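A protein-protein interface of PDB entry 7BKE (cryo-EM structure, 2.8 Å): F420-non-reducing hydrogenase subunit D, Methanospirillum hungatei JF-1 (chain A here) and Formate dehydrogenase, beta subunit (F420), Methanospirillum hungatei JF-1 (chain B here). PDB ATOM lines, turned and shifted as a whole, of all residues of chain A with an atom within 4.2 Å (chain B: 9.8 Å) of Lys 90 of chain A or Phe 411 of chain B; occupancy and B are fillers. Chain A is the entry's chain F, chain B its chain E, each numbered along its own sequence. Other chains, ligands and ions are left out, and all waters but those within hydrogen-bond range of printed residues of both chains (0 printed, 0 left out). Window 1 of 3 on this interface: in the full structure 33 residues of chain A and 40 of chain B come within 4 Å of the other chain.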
ATOM      1  N   MET A  86      10.297  -6.011  -6.877  1.00  0.00           N
ATOM      2  CA  MET A  86       9.478  -7.201  -7.094  1.00  0.00           C
ATOM      3  C   MET A  86       8.493  -7.452  -5.970  1.00  0.00           C
ATOM      4  O   MET A  86       7.411  -7.989  -6.223  1.00  0.00           O
ATOM      5  CB  MET A  86      10.339  -8.444  -7.309  1.00  0.00           C
ATOM      6  CG  MET A  86      11.499  -8.243  -8.237  1.00  0.00           C
ATOM      7  SD  MET A  86      11.002  -7.589  -9.838  1.00  0.00           S
ATOM      8  CE  MET A  86      12.534  -6.837 -10.369  1.00  0.00           C
ATOM      9  N   PHE A  87       8.822  -7.082  -4.737  1.00  0.00           N
ATOM     10  CA  PHE A  87       7.810  -7.113  -3.689  1.00  0.00           C
ATOM     11  C   PHE A  87       6.634  -6.222  -4.057  1.00  0.00           C
ATOM     12  O   PHE A  87       5.466  -6.636  -3.981  1.00  0.00           O
ATOM     13  CB  PHE A  87       8.421  -6.679  -2.364  1.00  0.00           C
ATOM     14  CG  PHE A  87       8.937  -7.805  -1.544  1.00  0.00           C
ATOM     15  CD1 PHE A  87       8.112  -8.833  -1.172  1.00  0.00           C
ATOM     16  CD2 PHE A  87      10.250  -7.839  -1.147  1.00  0.00           C
ATOM     17  CE1 PHE A  87       8.590  -9.870  -0.422  1.00  0.00           C
ATOM     18  CE2 PHE A  87      10.730  -8.871  -0.396  1.00  0.00           C
ATOM     19  CZ  PHE A  87       9.899  -9.887  -0.034  1.00  0.00           C
ATOM     20  N   MET A  88       6.925  -4.998  -4.500  1.00  0.00           N
ATOM     21  CA  MET A  88       5.847  -4.116  -4.929  1.00  0.00           C
ATOM     22  C   MET A  88       5.096  -4.662  -6.138  1.00  0.00           C
ATOM     23  O   MET A  88       3.884  -4.472  -6.243  1.00  0.00           O
ATOM     24  CB  MET A  88       6.387  -2.723  -5.218  1.00  0.00           C
ATOM     25  CG  MET A  88       5.312  -1.742  -5.605  1.00  0.00           C
ATOM     26  SD  MET A  88       5.889  -0.058  -5.779  1.00  0.00           S
ATOM     27  CE  MET A  88       4.424   0.723  -6.423  1.00  0.00           C
ATOM     28  N   ILE A  89       5.780  -5.337  -7.061  1.00  0.00           N
ATOM     29  CA  ILE A  89       5.082  -5.929  -8.201  1.00  0.00           C
ATOM     30  C   ILE A  89       4.147  -7.042  -7.768  1.00  0.00           C
ATOM     31  O   ILE A  89       3.050  -7.177  -8.309  1.00  0.00           O
ATOM     32  CB  ILE A  89       6.063  -6.425  -9.277  1.00  0.00           C
ATOM     33  CG1 ILE A  89       6.896  -5.276  -9.793  1.00  0.00           C
ATOM     34  CG2 ILE A  89       5.320  -7.060 -10.421  1.00  0.00           C
ATOM     35  CD1 ILE A  89       6.029  -4.237 -10.422  1.00  0.00           C
ATOM     36  N   LYS A  90       4.572  -7.838  -6.788  1.00  0.00           N
ATOM     37  CA  LYS A  90       3.704  -8.895  -6.231  1.00  0.00           C
ATOM     38  C   LYS A  90       2.434  -8.263  -5.681  1.00  0.00           C
ATOM     39  O   LYS A  90       1.358  -8.797  -5.976  1.00  0.00           O
ATOM     40  CB  LYS A  90       4.454  -9.719  -5.193  1.00  0.00           C
ATOM     41  CG  LYS A  90       5.675 -10.459  -5.704  1.00  0.00           C
ATOM     42  CD  LYS A  90       5.730 -11.889  -5.266  1.00  0.00           C
ATOM     43  CE  LYS A  90       4.694 -12.726  -5.970  1.00  0.00           C
ATOM     44  NZ  LYS A  90       4.999 -14.166  -5.861  1.00  0.00           N
ATOM     45  N   ASN A  91       2.555  -7.170  -4.943  1.00  0.00           N
ATOM     46  CA  ASN A  91       1.384  -6.451  -4.400  1.00  0.00           C
ATOM     47  C   ASN A  91       0.472  -5.928  -5.507  1.00  0.00           C
ATOM     48  O   ASN A  91      -0.690  -6.167  -5.412  1.00  0.00           O
ATOM     49  CB  ASN A  91       1.817  -5.362  -3.437  1.00  0.00           C
ATOM     50  CG  ASN A  91       0.965  -5.280  -2.196  1.00  0.00           C
ATOM     51  OD1 ASN A  91      -0.115  -5.856  -2.135  1.00  0.00           O
ATOM     52  ND2 ASN A  91       1.449  -4.566  -1.197  1.00  0.00           N
ATOM     53  N   LEU A  92       0.987  -5.333  -6.560  1.00  0.00           N
ATOM     54  CA  LEU A  92       0.174  -4.778  -7.650  1.00  0.00           C
ATOM     55  C   LEU A  92      -0.599  -5.887  -8.334  1.00  0.00           C
ATOM     56  O   LEU A  92      -1.754  -5.660  -8.628  1.00  0.00           O
ATOM     57  CB  LEU A  92       1.138  -4.120  -8.635  1.00  0.00           C
ATOM     58  CG  LEU A  92       0.604  -3.010  -9.531  1.00  0.00           C
ATOM     59  CD1 LEU A  92       1.674  -1.951  -9.689  1.00  0.00           C
ATOM     60  CD2 LEU A  92       0.217  -3.559 -10.894  1.00  0.00           C
ATOM     61  N   LEU A  93       0.020  -7.022  -8.619  1.00  0.00           N
ATOM     62  CA  LEU A  93      -0.663  -8.095  -9.375  1.00  0.00           C
ATOM     63  C   LEU A  93      -1.782  -8.679  -8.528  1.00  0.00           C
ATOM     64  O   LEU A  93      -2.806  -8.998  -9.098  1.00  0.00           O
ATOM     65  CB  LEU A  93       0.342  -9.143  -9.835  1.00  0.00           C
ATOM     66  CG  LEU A  93       1.450  -8.670 -10.767  1.00  0.00           C
ATOM     67  CD1 LEU A  93       2.614  -9.640 -10.712  1.00  0.00           C
ATOM     68  CD2 LEU A  93       0.936  -8.530 -12.187  1.00  0.00           C
ATOM     69  N   ARG A  94      -1.577  -8.803  -7.222  1.00  0.00           N
ATOM     70  CA  ARG A  94      -2.624  -9.295  -6.297  1.00  0.00           C
ATOM     71  C   ARG A  94      -3.815  -8.348  -6.299  1.00  0.00           C
ATOM     72  O   ARG A  94      -4.924  -8.854  -6.222  1.00  0.00           O
ATOM     73  CB  ARG A  94      -2.053  -9.381  -4.882  1.00  0.00           C
ATOM     74  CG  ARG A  94      -2.838 -10.259  -3.927  1.00  0.00           C
ATOM     75  CD  ARG A  94      -2.710  -9.706  -2.527  1.00  0.00           C
ATOM     76  NE  ARG A  94      -2.920 -10.753  -1.542  1.00  0.00           N
ATOM     77  CZ  ARG A  94      -3.978 -10.828  -0.751  1.00  0.00           C
ATOM     78  NH1 ARG A  94      -4.925  -9.910  -0.824  1.00  0.00           N
ATOM     79  NH2 ARG A  94      -4.082 -11.818   0.114  1.00  0.00           N
ATOM     80  N   ASP A 100      -0.803 -13.648  -8.228  1.00  0.00           N
ATOM     81  CA  ASP A 100       0.581 -13.161  -7.956  1.00  0.00           C
ATOM     82  C   ASP A 100       1.609 -14.277  -7.967  1.00  0.00           C
ATOM     83  O   ASP A 100       2.777 -13.951  -8.015  1.00  0.00           O
ATOM     84  CB  ASP A 100       0.675 -12.369  -6.656  1.00  0.00           C
ATOM     85  CG  ASP A 100       0.526 -13.176  -5.381  1.00  0.00           C
ATOM     86  OD1 ASP A 100      -0.589 -13.202  -4.836  1.00  0.00           O
ATOM     87  OD2 ASP A 100       1.531 -13.749  -4.929  1.00  0.00           O
ATOM     88  N   PHE A 103       4.390 -14.789 -10.722  1.00  0.00           N
ATOM     89  CA  PHE A 103       5.645 -14.062 -10.691  1.00  0.00           C
ATOM     90  C   PHE A 103       6.444 -14.483  -9.472  1.00  0.00           C
ATOM     91  O   PHE A 103       5.886 -14.663  -8.390  1.00  0.00           O
ATOM     92  CB  PHE A 103       5.401 -12.555 -10.657  1.00  0.00           C
ATOM     93  CG  PHE A 103       6.649 -11.754 -10.506  1.00  0.00           C
ATOM     94  CD1 PHE A 103       7.514 -11.595 -11.561  1.00  0.00           C
ATOM     95  CD2 PHE A 103       6.972 -11.185  -9.296  1.00  0.00           C
ATOM     96  CE1 PHE A 103       8.663 -10.883 -11.415  1.00  0.00           C
ATOM     97  CE2 PHE A 103       8.122 -10.477  -9.156  1.00  0.00           C
ATOM     98  CZ  PHE A 103       8.969 -10.326 -10.214  1.00  0.00           C
ATOM     99  N   LYS B 278     -12.835  -9.080  -6.136  1.00  0.00           N
ATOM    100  CA  LYS B 278     -11.602  -9.800  -5.750  1.00  0.00           C
ATOM    101  C   LYS B 278     -11.289 -10.778  -6.875  1.00  0.00           C
ATOM    102  O   LYS B 278     -12.231 -11.192  -7.555  1.00  0.00           O
ATOM    103  CB  LYS B 278     -11.852 -10.608  -4.478  1.00  0.00           C
ATOM    104  CG  LYS B 278     -12.020  -9.807  -3.198  1.00  0.00           C
ATOM    105  CD  LYS B 278     -11.065 -10.229  -2.101  1.00  0.00           C
ATOM    106  CE  LYS B 278      -9.873  -9.306  -1.970  1.00  0.00           C
ATOM    107  NZ  LYS B 278      -8.626 -10.062  -1.723  1.00  0.00           N
ATOM    108  N   GLN B 365      -4.871   0.307  -4.262  1.00  0.00           N
ATOM    109  CA  GLN B 365      -3.514  -0.230  -4.263  1.00  0.00           C
ATOM    110  C   GLN B 365      -2.632   0.441  -3.219  1.00  0.00           C
ATOM    111  O   GLN B 365      -1.797  -0.216  -2.580  1.00  0.00           O
ATOM    112  CB  GLN B 365      -2.932  -0.072  -5.651  1.00  0.00           C
ATOM    113  CG  GLN B 365      -3.675  -0.929  -6.617  1.00  0.00           C
ATOM    114  CD  GLN B 365      -3.168  -0.797  -7.996  1.00  0.00           C
ATOM    115  OE1 GLN B 365      -2.278  -0.002  -8.262  1.00  0.00           O
ATOM    116  NE2 GLN B 365      -3.750  -1.551  -8.910  1.00  0.00           N
ATOM    117  N   GLU B 368      -2.590  -0.686   0.784  1.00  0.00           N
ATOM    118  CA  GLU B 368      -1.836  -1.840   1.220  1.00  0.00           C
ATOM    119  C   GLU B 368      -0.385  -1.824   0.769  1.00  0.00           C
ATOM    120  O   GLU B 368       0.435  -2.497   1.387  1.00  0.00           O
ATOM    121  CB  GLU B 368      -2.537  -3.091   0.781  1.00  0.00           C
ATOM    122  CG  GLU B 368      -2.487  -3.333  -0.625  1.00  0.00           C
ATOM    123  CD  GLU B 368      -3.482  -4.369  -0.948  1.00  0.00           C
ATOM    124  OE1 GLU B 368      -4.439  -4.536  -0.173  1.00  0.00           O
ATOM    125  OE2 GLU B 368      -3.252  -5.102  -1.896  1.00  0.00           O
ATOM    126  N   ILE B 369      -0.013  -1.040  -0.246  1.00  0.00           N
ATOM    127  CA  ILE B 369       1.408  -0.714  -0.330  1.00  0.00           C
ATOM    128  C   ILE B 369       1.851  -0.049   0.965  1.00  0.00           C
ATOM    129  O   ILE B 369       2.971  -0.262   1.444  1.00  0.00           O
ATOM    130  CB  ILE B 369       1.712   0.185  -1.544  1.00  0.00           C
ATOM    131  CG1 ILE B 369       1.504  -0.557  -2.856  1.00  0.00           C
ATOM    132  CG2 ILE B 369       3.126   0.690  -1.485  1.00  0.00           C
ATOM    133  CD1 ILE B 369       2.571  -1.557  -3.142  1.00  0.00           C
ATOM    134  N   LYS B 371       0.417  -0.546   4.093  1.00  0.00           N
ATOM    135  CA  LYS B 371       0.550  -1.510   5.184  1.00  0.00           C
ATOM    136  C   LYS B 371       1.612  -2.570   4.913  1.00  0.00           C
ATOM    137  O   LYS B 371       1.943  -3.335   5.824  1.00  0.00           O
ATOM    138  CB  LYS B 371      -0.779  -2.194   5.496  1.00  0.00           C
ATOM    139  CG  LYS B 371      -1.253  -3.157   4.451  1.00  0.00           C
ATOM    140  CD  LYS B 371      -2.511  -3.856   4.919  1.00  0.00           C
ATOM    141  CE  LYS B 371      -3.238  -4.564   3.786  1.00  0.00           C
ATOM    142  NZ  LYS B 371      -2.437  -5.621   3.112  1.00  0.00           N
ATOM    143  N   MET B 372       2.148  -2.635   3.700  1.00  0.00           N
ATOM    144  CA  MET B 372       3.292  -3.482   3.392  1.00  0.00           C
ATOM    145  C   MET B 372       4.612  -2.821   3.770  1.00  0.00           C
ATOM    146  O   MET B 372       5.391  -3.378   4.543  1.00  0.00           O
ATOM    147  CB  MET B 372       3.307  -3.805   1.904  1.00  0.00           C
ATOM    148  CG  MET B 372       4.451  -4.672   1.495  1.00  0.00           C
ATOM    149  SD  MET B 372       4.297  -5.241  -0.203  1.00  0.00           S
ATOM    150  CE  MET B 372       5.626  -6.415  -0.231  1.00  0.00           C
ATOM    151  N   PHE B 373       4.875  -1.631   3.233  1.00  0.00           N
ATOM    152  CA  PHE B 373       6.151  -0.970   3.437  1.00  0.00           C
ATOM    153  C   PHE B 373       6.142   0.034   4.579  1.00  0.00           C
ATOM    154  O   PHE B 373       7.215   0.442   5.025  1.00  0.00           O
ATOM    155  CB  PHE B 373       6.594  -0.265   2.155  1.00  0.00           C
ATOM    156  CG  PHE B 373       6.900  -1.203   1.029  1.00  0.00           C
ATOM    157  CD1 PHE B 373       8.116  -1.833   0.952  1.00  0.00           C
ATOM    158  CD2 PHE B 373       5.976  -1.440   0.039  1.00  0.00           C
ATOM    159  CE1 PHE B 373       8.393  -2.689  -0.077  1.00  0.00           C
ATOM    160  CE2 PHE B 373       6.258  -2.293  -0.989  1.00  0.00           C
ATOM    161  CZ  PHE B 373       7.468  -2.915  -1.046  1.00  0.00           C
ATOM    162  N   HIS B 386      11.088   3.545  -3.515  1.00  0.00           N
ATOM    163  CA  HIS B 386      12.077   3.121  -4.490  1.00  0.00           C
ATOM    164  C   HIS B 386      13.197   4.122  -4.677  1.00  0.00           C
ATOM    165  O   HIS B 386      14.213   3.781  -5.279  1.00  0.00           O
ATOM    166  CB  HIS B 386      11.395   2.844  -5.820  1.00  0.00           C
ATOM    167  CG  HIS B 386      10.390   1.749  -5.732  1.00  0.00           C
ATOM    168  ND1 HIS B 386      10.635   0.586  -5.039  1.00  0.00           N
ATOM    169  CD2 HIS B 386       9.127   1.655  -6.195  1.00  0.00           C
ATOM    170  CE1 HIS B 386       9.574  -0.191  -5.102  1.00  0.00           C
ATOM    171  NE2 HIS B 386       8.641   0.439  -5.790  1.00  0.00           N
ATOM    172  N   ARG B 397      12.821  -8.098   5.049  1.00  0.00           N
ATOM    173  CA  ARG B 397      11.585  -8.545   4.373  1.00  0.00           C
ATOM    174  C   ARG B 397      11.815  -9.912   3.747  1.00  0.00           C
ATOM    175  O   ARG B 397      10.861 -10.636   3.597  1.00  0.00           O
ATOM    176  CB  ARG B 397      11.208  -7.485   3.348  1.00  0.00           C
ATOM    177  CG  ARG B 397       9.731  -7.454   2.986  1.00  0.00           C
ATOM    178  CD  ARG B 397       9.266  -6.112   2.453  1.00  0.00           C
ATOM    179  NE  ARG B 397      10.364  -5.201   2.186  1.00  0.00           N
ATOM    180  CZ  ARG B 397      10.488  -4.003   2.739  1.00  0.00           C
ATOM    181  NH1 ARG B 397       9.574  -3.575   3.590  1.00  0.00           N
ATOM    182  NH2 ARG B 397      11.526  -3.239   2.440  1.00  0.00           N
ATOM    183  N   LEU B 398      13.041 -10.238   3.360  1.00  0.00           N
ATOM    184  CA  LEU B 398      13.301 -11.576   2.851  1.00  0.00           C
ATOM    185  C   LEU B 398      13.300 -12.599   3.980  1.00  0.00           C
ATOM    186  O   LEU B 398      12.794 -13.712   3.812  1.00  0.00           O
ATOM    187  CB  LEU B 398      14.616 -11.623   2.087  1.00  0.00           C
ATOM    188  CG  LEU B 398      14.698 -12.924   1.300  1.00  0.00           C
ATOM    189  CD1 LEU B 398      13.694 -12.887   0.177  1.00  0.00           C
ATOM    190  CD2 LEU B 398      16.082 -13.158   0.763  1.00  0.00           C
ATOM    191  N   ALA B 400      11.643 -12.267   6.848  1.00  0.00           N
ATOM    192  CA  ALA B 400      10.281 -12.369   7.359  1.00  0.00           C
ATOM    193  C   ALA B 400       9.435 -13.314   6.523  1.00  0.00           C
ATOM    194  O   ALA B 400       8.533 -13.968   7.055  1.00  0.00           O
ATOM    195  CB  ALA B 400       9.631 -10.988   7.412  1.00  0.00           C
ATOM    196  N   THR B 401       9.695 -13.401   5.219  1.00  0.00           N
ATOM    197  CA  THR B 401       8.970 -14.406   4.441  1.00  0.00           C
ATOM    198  C   THR B 401       9.369 -15.828   4.813  1.00  0.00           C
ATOM    199  O   THR B 401       8.662 -16.768   4.445  1.00  0.00           O
ATOM    200  CB  THR B 401       9.176 -14.210   2.941  1.00  0.00           C
ATOM    201  OG1 THR B 401      10.575 -14.142   2.648  1.00  0.00           O
ATOM    202  CG2 THR B 401       8.500 -12.946   2.472  1.00  0.00           C
ATOM    203  N   THR B 403      11.727 -17.662   3.596  1.00  0.00           N
ATOM    204  CA  THR B 403      11.781 -18.354   2.319  1.00  0.00           C
ATOM    205  C   THR B 403      13.057 -17.924   1.612  1.00  0.00           C
ATOM    206  O   THR B 403      13.637 -16.883   1.925  1.00  0.00           O
ATOM    207  CB  THR B 403      10.524 -18.037   1.494  1.00  0.00           C
ATOM    208  OG1 THR B 403       9.367 -18.399   2.258  1.00  0.00           O
ATOM    209  CG2 THR B 403      10.482 -18.826   0.196  1.00  0.00           C
ATOM    210  N   SER B 405      13.274 -17.214  -1.581  1.00  0.00           N
ATOM    211  CA  SER B 405      12.988 -16.437  -2.774  1.00  0.00           C
ATOM    212  C   SER B 405      11.870 -15.457  -2.458  1.00  0.00           C
ATOM    213  O   SER B 405      11.474 -15.290  -1.303  1.00  0.00           O
ATOM    214  CB  SER B 405      12.619 -17.356  -3.941  1.00  0.00           C
ATOM    215  OG  SER B 405      11.465 -18.104  -3.639  1.00  0.00           O
ATOM    216  N   ILE B 406      11.373 -14.792  -3.491  1.00  0.00           N
ATOM    217  CA  ILE B 406      10.185 -13.972  -3.346  1.00  0.00           C
ATOM    218  C   ILE B 406       9.070 -14.688  -4.083  1.00  0.00           C
ATOM    219  O   ILE B 406       8.832 -14.433  -5.265  1.00  0.00           O
ATOM    220  CB  ILE B 406      10.441 -12.554  -3.887  1.00  0.00           C
ATOM    221  CG1 ILE B 406      11.562 -11.890  -3.090  1.00  0.00           C
ATOM    222  CG2 ILE B 406       9.189 -11.706  -3.843  1.00  0.00           C
ATOM    223  CD1 ILE B 406      11.854 -10.489  -3.490  1.00  0.00           C
ATOM    224  N   TYR B 407       8.392 -15.612  -3.408  1.00  0.00           N
ATOM    225  CA  TYR B 407       7.345 -16.365  -4.079  1.00  0.00           C
ATOM    226  C   TYR B 407       6.039 -16.437  -3.294  1.00  0.00           C
ATOM    227  O   TYR B 407       4.970 -16.206  -3.862  1.00  0.00           O
ATOM    228  CB  TYR B 407       7.861 -17.772  -4.374  1.00  0.00           C
ATOM    229  CG  TYR B 407       6.838 -18.713  -4.928  1.00  0.00           C
ATOM    230  CD1 TYR B 407       6.068 -18.374  -6.020  1.00  0.00           C
ATOM    231  CD2 TYR B 407       6.634 -19.942  -4.340  1.00  0.00           C
ATOM    232  CE1 TYR B 407       5.133 -19.241  -6.518  1.00  0.00           C
ATOM    233  CE2 TYR B 407       5.703 -20.809  -4.824  1.00  0.00           C
ATOM    234  CZ  TYR B 407       4.952 -20.459  -5.911  1.00  0.00           C
ATOM    235  OH  TYR B 407       4.019 -21.346  -6.384  1.00  0.00           O
ATOM    236  N   THR B 408       6.106 -16.709  -1.987  1.00  0.00           N
ATOM    237  CA  THR B 408       4.912 -16.940  -1.173  1.00  0.00           C
ATOM    238  C   THR B 408       5.209 -16.577   0.275  1.00  0.00           C
ATOM    239  O   THR B 408       6.307 -16.130   0.607  1.00  0.00           O
ATOM    240  CB  THR B 408       4.416 -18.391  -1.242  1.00  0.00           C
ATOM    241  OG1 THR B 408       5.512 -19.293  -1.051  1.00  0.00           O
ATOM    242  CG2 THR B 408       3.723 -18.690  -2.557  1.00  0.00           C
ATOM    243  N   ASN B 409       4.207 -16.773   1.140  1.00  0.00           N
ATOM    244  CA  ASN B 409       4.280 -16.400   2.557  1.00  0.00           C
ATOM    245  C   ASN B 409       4.593 -14.924   2.735  1.00  0.00           C
ATOM    246  O   ASN B 409       5.254 -14.534   3.694  1.00  0.00           O
ATOM    247  CB  ASN B 409       5.296 -17.250   3.322  1.00  0.00           C
ATOM    248  CG  ASN B 409       4.943 -18.715   3.331  1.00  0.00           C
ATOM    249  OD1 ASN B 409       4.586 -19.285   2.308  1.00  0.00           O
ATOM    250  ND2 ASN B 409       5.095 -19.347   4.483  1.00  0.00           N
ATOM    251  N   ILE B 410       4.057 -14.116   1.811  1.00  0.00           N
ATOM    252  CA  ILE B 410       4.247 -12.635   1.813  1.00  0.00           C
ATOM    253  C   ILE B 410       2.941 -11.976   2.280  1.00  0.00           C
ATOM    254  O   ILE B 410       3.005 -10.963   2.985  1.00  0.00           O
ATOM    255  CB  ILE B 410       4.570 -12.168   0.380  1.00  0.00           C
ATOM    256  CG1 ILE B 410       5.788 -12.870  -0.220  1.00  0.00           C
ATOM    257  CG2 ILE B 410       4.698 -10.657   0.303  1.00  0.00           C
ATOM    258  CD1 ILE B 410       5.901 -12.702  -1.709  1.00  0.00           C
ATOM    259  N   PHE B 411       1.787 -12.541   1.904  1.00  0.00           N
ATOM    260  CA  PHE B 411       0.488 -11.923   2.276  1.00  0.00           C
ATOM    261  C   PHE B 411      -0.367 -12.817   3.181  1.00  0.00           C
ATOM    262  O   PHE B 411      -0.079 -14.027   3.200  1.00  0.00           O
ATOM    263  CB  PHE B 411      -0.318 -11.670   1.003  1.00  0.00           C
ATOM    264  CG  PHE B 411       0.373 -10.897  -0.089  1.00  0.00           C
ATOM    265  CD1 PHE B 411       0.578 -11.469  -1.334  1.00  0.00           C
ATOM    266  CD2 PHE B 411       0.794  -9.596   0.118  1.00  0.00           C
ATOM    267  CE1 PHE B 411       1.208 -10.759  -2.341  1.00  0.00           C
ATOM    268  CE2 PHE B 411       1.420  -8.886  -0.894  1.00  0.00           C
ATOM    269  CZ  PHE B 411       1.626  -9.470  -2.118  1.00  0.00           C
ATOM    270  N   THR B 412      -1.334 -12.256   3.940  1.00  0.00           N
ATOM    271  CA  THR B 412      -2.337 -12.996   4.687  1.00  0.00           C
ATOM    272  C   THR B 412      -3.722 -12.918   4.049  1.00  0.00           C
ATOM    273  O   THR B 412      -3.961 -12.113   3.151  1.00  0.00           O
ATOM    274  CB  THR B 412      -2.411 -12.474   6.132  1.00  0.00           C
ATOM    275  OG1 THR B 412      -1.224 -12.856   6.837  1.00  0.00           O
ATOM    276  CG2 THR B 412      -3.623 -13.038   6.841  1.00  0.00           C
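The side-chain sulfur (SD) of Met 88 of chain A sits at hydrogen-bond distance from a ring nitrogen (NE2) of His 386 of chain B, at 2.8 Å. NZ of Lys 90 of chain A sits at hydrogen-bond distance from O of Tyr 407 of chain B (2.9 Å). The side-chain amide oxygen of Asn 91 of chain A lies close to the side-chain carboxylate of Glu 368 of chain B (3.2 Å). The side-chain amide nitrogen of Asn 91 of chain A lies within hydrogen-bond range of the side-chain sulfur of Met 372 of chain B. The backbone carbonyl oxygen (O) of Thr 412 of chain B is in hydrogen-bond range of the guanidinium group (NH2) of Arg 94 of chain A (3.1 Å).
The side-chain amino group (NZ) of Lys 90 of chain A is in salt-bridge range of the side-chain carboxylate (OD2) of Asp 100 of chain A, 3.6 Å away. NZ of Lys 90 of chain A lies within hydrogen-bond range of O of Phe 103 of chain A (2.7 Å). OE1 of Glu 368 of chain B is in salt-bridge range of NZ of Lys 371 of chain B.
Among the printed residues, merely in contact across the chains: Phe 87 of chain A with Met 372 of chain B (3.5 Å), Phe 87 of chain A with Arg 397 of chain B (3.8 Å), Phe 87 of chain A with Ile 406 of chain B (3.7 Å), Met 88 of chain A with Ile 369 of chain B (3.7 Å), Lys 90 of chain A with Ile 406 of chain B (3.7 Å), Lys 90 of chain A with Ile 410 of chain B (3.7 Å), Lys 90 of chain A with Phe 411 of chain B (3.8 Å), Asn 91 of chain A with Ile 369 of chain B (3.8 Å), Asn 91 of chain A with Phe 411 of chain B (3.6 Å), Arg 94 of chain A with Lys 278 of chain B (3.8 Å), Arg 94 of chain A with Phe 411 of chain B (3.6 Å) and Asp 100 of chain A with Phe 411 of chain B (3.9 Å).
Printed residues of chain B within 4 Å of Phe 87 of chain A: Met 372, Arg 397 and Ile 406. No residue of chain B comes within 4 Å of Ile 89 of chain A. Lys 90 of chain A touches just these residues of chain B: Ile 406 (3.7 Å), Tyr 407 (2.9 Å), Ile 410 (3.7 Å) and Phe 411 (3.8 Å). Asn 91 of chain A touches four residues of chain B. Phe 103 of chain A touches none of the printed residues of chain B. Phe 373 of chain B touches none of the printed residues of chain A. Printed residues of chain A within 4 Å of Arg 397 of chain B: Phe 87 (3.8 Å). Phe 411 of chain B touches just these residues of chain A: Lys 90 (3.8 Å), Asn 91 (3.6 Å), Arg 94 (3.6 Å) and Asp 100 (3.9 Å). The nearest residue of chain B that does not touch Lys 90 of chain A is Thr 408 of chain B (4.8 Å). The nearest printed residue of chain A that does not touch Ile 406 of chain B is Phe 103 of chain A (4.3 Å).
Of the 21 printed residues of chain B, 11 touch a printed residue of chain A. Hydrophobic or aromatic side chains of chain B that line the printed part of chain A: Ile 369, Met 372, His 386, Ile 406, Ile 410 and Phe 411. Of the 11 printed residues of chain A, 6 touch a printed residue of chain B. Among the printed residues, no Asp or Glu carboxylate lies within 4 Å of a Lys or Arg side-chain nitrogen of the other chain.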
